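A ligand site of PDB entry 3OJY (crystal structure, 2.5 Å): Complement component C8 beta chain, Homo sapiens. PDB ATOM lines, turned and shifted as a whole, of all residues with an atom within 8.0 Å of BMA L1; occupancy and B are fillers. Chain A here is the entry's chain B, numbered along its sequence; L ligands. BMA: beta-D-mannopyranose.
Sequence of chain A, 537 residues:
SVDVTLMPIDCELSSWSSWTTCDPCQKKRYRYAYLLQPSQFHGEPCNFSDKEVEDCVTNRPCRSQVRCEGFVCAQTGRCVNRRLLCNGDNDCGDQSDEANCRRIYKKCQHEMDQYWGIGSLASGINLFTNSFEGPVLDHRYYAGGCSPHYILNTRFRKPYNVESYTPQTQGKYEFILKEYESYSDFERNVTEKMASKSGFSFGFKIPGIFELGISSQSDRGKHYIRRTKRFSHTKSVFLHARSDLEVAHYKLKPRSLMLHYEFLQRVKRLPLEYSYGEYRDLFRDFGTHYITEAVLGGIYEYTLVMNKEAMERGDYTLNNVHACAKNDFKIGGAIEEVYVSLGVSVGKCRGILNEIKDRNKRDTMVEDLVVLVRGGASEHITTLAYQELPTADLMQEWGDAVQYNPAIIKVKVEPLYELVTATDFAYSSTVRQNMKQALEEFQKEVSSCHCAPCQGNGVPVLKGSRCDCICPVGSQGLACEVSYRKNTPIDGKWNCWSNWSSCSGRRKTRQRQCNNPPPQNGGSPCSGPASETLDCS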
ATOM      1  N   TRP A  16      15.958 -20.930  26.845  1.00  0.00           N
ATOM      2  CA  TRP A  16      15.313 -19.756  26.296  1.00  0.00           C
ATOM      3  C   TRP A  16      15.698 -19.527  24.834  1.00  0.00           C
ATOM      4  O   TRP A  16      16.864 -19.547  24.492  1.00  0.00           O
ATOM      5  CB  TRP A  16      15.786 -18.638  27.213  1.00  0.00           C
ATOM      6  CG  TRP A  16      15.152 -18.623  28.593  1.00  0.00           C
ATOM      7  CD1 TRP A  16      15.762 -18.698  29.957  1.00  0.00           C
ATOM      8  CD2 TRP A  16      13.775 -18.511  28.862  1.00  0.00           C
ATOM      9  NE1 TRP A  16      14.746 -18.612  30.846  1.00  0.00           N
ATOM     10  CE2 TRP A  16      13.556 -18.506  30.235  1.00  0.00           C
ATOM     11  CE3 TRP A  16      12.699 -18.430  27.992  1.00  0.00           C
ATOM     12  CZ2 TRP A  16      12.277 -18.427  30.763  1.00  0.00           C
ATOM     13  CZ3 TRP A  16      11.417 -18.337  28.521  1.00  0.00           C
ATOM     14  CH2 TRP A  16      11.185 -18.329  29.900  1.00  0.00           C
ATOM     15  N   SER A  17      14.710 -19.359  23.963  1.00  0.00           N
ATOM     16  CA  SER A  17      14.900 -18.823  22.604  1.00  0.00           C
ATOM     17  C   SER A  17      15.604 -17.456  22.632  1.00  0.00           C
ATOM     18  O   SER A  17      15.447 -16.697  23.578  1.00  0.00           O
ATOM     19  CB  SER A  17      13.541 -18.595  21.941  1.00  0.00           C
ATOM     20  OG  SER A  17      13.001 -17.358  22.363  1.00  0.00           O
ATOM     21  N   SER A  18      16.363 -17.165  21.588  1.00  0.00           N
ATOM     22  CA  SER A  18      16.926 -15.837  21.379  1.00  0.00           C
ATOM     23  C   SER A  18      15.812 -14.787  21.521  1.00  0.00           C
ATOM     24  O   SER A  18      14.723 -14.975  20.995  1.00  0.00           O
ATOM     25  CB  SER A  18      17.530 -15.834  19.975  1.00  0.00           C
ATOM     26  OG  SER A  18      17.981 -14.560  19.591  1.00  0.00           O
ATOM     27  N   TRP A  19      16.071 -13.707  22.237  1.00  0.00           N
ATOM     28  CA  TRP A  19      15.075 -12.637  22.438  1.00  0.00           C
ATOM     29  C   TRP A  19      14.648 -12.097  21.098  1.00  0.00           C
ATOM     30  O   TRP A  19      15.426 -12.121  20.146  1.00  0.00           O
ATOM     31  CB  TRP A  19      15.781 -11.472  23.143  1.00  0.00           C
ATOM     32  CG  TRP A  19      15.747 -11.479  24.665  1.00  0.00           C
ATOM     33  CD1 TRP A  19      16.884 -11.557  25.623  1.00  0.00           C
ATOM     34  CD2 TRP A  19      14.639 -11.378  25.492  1.00  0.00           C
ATOM     35  NE1 TRP A  19      16.384 -11.498  26.856  1.00  0.00           N
ATOM     36  CE2 TRP A  19      15.055 -11.401  26.831  1.00  0.00           C
ATOM     37  CE3 TRP A  19      13.291 -11.299  25.187  1.00  0.00           C
ATOM     38  CZ2 TRP A  19      14.148 -11.332  27.881  1.00  0.00           C
ATOM     39  CZ3 TRP A  19      12.381 -11.225  26.245  1.00  0.00           C
ATOM     40  CH2 TRP A  19      12.797 -11.240  27.578  1.00  0.00           C
ATOM     41  N   THR A  20      13.410 -11.607  20.982  1.00  0.00           N
ATOM     42  CA  THR A  20      13.040 -10.851  19.783  1.00  0.00           C
ATOM     43  C   THR A  20      13.492  -9.405  19.911  1.00  0.00           C
ATOM     44  O   THR A  20      13.632  -8.868  21.021  1.00  0.00           O
ATOM     45  CB  THR A  20      11.535 -10.828  19.559  1.00  0.00           C
ATOM     46  OG1 THR A  20      10.909 -10.187  20.660  1.00  0.00           O
ATOM     47  CG2 THR A  20      11.016 -12.229  19.410  1.00  0.00           C
ATOM     48  N   THR A  21      13.696  -8.748  18.769  1.00  0.00           N
ATOM     49  CA  THR A  21      13.969  -7.305  18.775  1.00  0.00           C
ATOM     50  C   THR A  21      12.693  -6.566  19.140  1.00  0.00           C
ATOM     51  O   THR A  21      11.610  -7.092  18.898  1.00  0.00           O
ATOM     52  CB  THR A  21      14.498  -6.777  17.415  1.00  0.00           C
ATOM     53  OG1 THR A  21      15.132  -5.503  17.624  1.00  0.00           O
ATOM     54  CG2 THR A  21      13.357  -6.639  16.387  1.00  0.00           C
ATOM     55  N   ARG A  29      10.198  -6.852  24.042  1.00  0.00           N
ATOM     56  CA  ARG A  29      10.793  -8.065  23.430  1.00  0.00           C
ATOM     57  C   ARG A  29      10.342  -9.328  24.170  1.00  0.00           C
ATOM     58  O   ARG A  29      10.076  -9.281  25.364  1.00  0.00           O
ATOM     59  CB  ARG A  29      12.331  -7.961  23.304  1.00  0.00           C
ATOM     60  CG  ARG A  29      13.086  -7.813  24.580  1.00  0.00           C
ATOM     61  CD  ARG A  29      14.241  -6.872  24.422  1.00  0.00           C
ATOM     62  NE  ARG A  29      15.332  -7.190  25.339  1.00  0.00           N
ATOM     63  CZ  ARG A  29      16.514  -7.672  24.973  1.00  0.00           C
ATOM     64  NH1 ARG A  29      16.803  -7.863  23.683  1.00  0.00           N
ATOM     65  NH2 ARG A  29      17.419  -7.979  25.910  1.00  0.00           N
ATOM     66  N   TYR A  30      10.271 -10.435  23.446  1.00  0.00           N
ATOM     67  CA  TYR A  30       9.803 -11.727  23.992  1.00  0.00           C
ATOM     68  C   TYR A  30      10.751 -12.854  23.695  1.00  0.00           C
ATOM     69  O   TYR A  30      11.473 -12.812  22.700  1.00  0.00           O
ATOM     70  CB  TYR A  30       8.483 -12.096  23.359  1.00  0.00           C
ATOM     71  CG  TYR A  30       7.575 -10.926  23.304  1.00  0.00           C
ATOM     72  CD1 TYR A  30       7.636 -10.012  22.230  1.00  0.00           C
ATOM     73  CD2 TYR A  30       6.670 -10.705  24.309  1.00  0.00           C
ATOM     74  CE1 TYR A  30       6.773  -8.913  22.179  1.00  0.00           C
ATOM     75  CE2 TYR A  30       5.817  -9.620  24.272  1.00  0.00           C
ATOM     76  CZ  TYR A  30       5.871  -8.738  23.205  1.00  0.00           C
ATOM     77  OH  TYR A  30       5.028  -7.665  23.220  1.00  0.00           O
ATOM     78  N   ARG A  31      10.742 -13.867  24.564  1.00  0.00           N
ATOM     79  CA  ARG A  31      11.550 -15.100  24.364  1.00  0.00           C
ATOM     80  C   ARG A  31      10.728 -16.252  24.990  1.00  0.00           C
ATOM     81  O   ARG A  31       9.827 -16.003  25.795  1.00  0.00           O
ATOM     82  CB  ARG A  31      12.910 -14.982  25.077  1.00  0.00           C
ATOM     83  CG  ARG A  31      12.776 -15.193  26.576  1.00  0.00           C
ATOM     84  CD  ARG A  31      13.777 -14.507  27.499  1.00  0.00           C
ATOM     85  NE  ARG A  31      15.140 -14.906  27.262  1.00  0.00           N
ATOM     86  CZ  ARG A  31      16.078 -15.022  28.205  1.00  0.00           C
ATOM     87  NH1 ARG A  31      15.774 -14.833  29.476  1.00  0.00           N
ATOM     88  NH2 ARG A  31      17.336 -15.387  27.862  1.00  0.00           N
ATOM     89  N   GLU A  52       9.075 -15.138  28.875  1.00  0.00           N
ATOM     90  CA  GLU A  52       9.315 -13.869  29.512  1.00  0.00           C
ATOM     91  C   GLU A  52       8.958 -12.746  28.546  1.00  0.00           C
ATOM     92  O   GLU A  52       8.981 -12.930  27.339  1.00  0.00           O
ATOM     93  CB  GLU A  52      10.779 -13.727  29.847  1.00  0.00           C
ATOM     94  CG  GLU A  52      11.325 -14.721  30.797  1.00  0.00           C
ATOM     95  CD  GLU A  52      12.589 -14.185  31.390  1.00  0.00           C
ATOM     96  OE1 GLU A  52      13.662 -14.724  31.084  1.00  0.00           O
ATOM     97  OE2 GLU A  52      12.509 -13.157  32.109  1.00  0.00           O
ATOM     98  N   GLU A  54      10.258  -8.581  28.060  1.00  0.00           N
ATOM     99  CA  GLU A  54      11.067  -7.443  28.554  1.00  0.00           C
ATOM    100  C   GLU A  54      10.498  -6.117  28.044  1.00  0.00           C
ATOM    101  O   GLU A  54      10.017  -6.043  26.913  1.00  0.00           O
ATOM    102  CB  GLU A  54      12.546  -7.546  28.125  1.00  0.00           C
ATOM    103  CG  GLU A  54      13.489  -8.333  29.047  1.00  0.00           C
ATOM    104  CD  GLU A  54      13.824  -7.641  30.384  1.00  0.00           C
ATOM    105  OE1 GLU A  54      14.254  -6.447  30.386  1.00  0.00           O
ATOM    106  OE2 GLU A  54      13.676  -8.310  31.441  1.00  0.00           O
HETATM  107  C1  BMA L   1      18.347 -11.621  25.470  1.00  0.00           C
HETATM  108  C2  BMA L   1      18.995 -12.854  24.830  1.00  0.00           C
HETATM  109  C3  BMA L   1      20.521 -12.613  24.925  1.00  0.00           C
HETATM  110  C4  BMA L   1      20.852 -11.291  24.237  1.00  0.00           C
HETATM  111  C5  BMA L   1      20.175 -10.183  25.046  1.00  0.00           C
HETATM  112  C6  BMA L   1      20.584  -8.740  24.692  1.00  0.00           C
HETATM  113  O2  BMA L   1      18.558 -13.068  23.472  1.00  0.00           O
HETATM  114  O3  BMA L   1      21.309 -13.719  24.458  1.00  0.00           O
HETATM  115  O4  BMA L   1      22.266 -11.072  24.134  1.00  0.00           O
HETATM  116  O5  BMA L   1      18.774 -10.384  24.883  1.00  0.00           O
HETATM  117  O6  BMA L   1      20.020  -8.283  23.461  1.00  0.00           O
HETATM  118  C1  BMA L   2      17.141 -18.805  30.529  1.00  0.00           C
HETATM  119  C2  BMA L   2      18.020 -20.018  30.201  1.00  0.00           C
HETATM  120  C3  BMA L   2      19.440 -19.568  29.973  1.00  0.00           C
HETATM  121  C4  BMA L   2      19.925 -18.584  31.030  1.00  0.00           C
HETATM  122  C5  BMA L   2      18.894 -17.479  31.296  1.00  0.00           C
HETATM  123  C6  BMA L   2      19.517 -16.100  31.140  1.00  0.00           C
HETATM  124  O2  BMA L   2      17.593 -20.741  29.044  1.00  0.00           O
HETATM  125  O3  BMA L   2      19.475 -18.932  28.687  1.00  0.00           O
HETATM  126  O4  BMA L   2      20.202 -19.275  32.250  1.00  0.00           O
HETATM  127  O5  BMA L   2      17.825 -17.584  30.342  1.00  0.00           O
HETATM  128  O6  BMA L   2      19.926 -16.002  29.769  1.00  0.00           O
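NH2 of Arg 31 is in hydrogen-bond range of O6 of BMA L2 (3.3 Å).
An oxygen (O2) of BMA L1 lies within hydrogen-bond range of the backbone NH (N) of Trp 19 (2.8 Å).
The guanidinium group (NH2) of Arg 29 is in hydrogen-bond range of an oxygen (O5) of BMA L1 (2.9 Å).
N of Trp 16 sits at hydrogen-bond distance from O2 of BMA L2.
CD1 of Trp 16 is covalently linked to C1 of BMA L2 (1.5 Å).
The aromatic ring (CD1) of Trp 19 is bonded to a carbon (C1) of BMA L1.
The backbone NH (N) of Glu 54 sits at hydrogen-bond distance from the backbone carbonyl oxygen (O) of Arg 29.
Merely in contact with BMA L1: Ser 18.
Hydrophobic or aromatic side chains that line BMA L1: Trp 19.
Within 4 Å of BMA L1: Ser 18, Trp 19 and Arg 29.
The nearest printed residue that does not touch BMA L1 is Arg 31 (4.3 Å).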
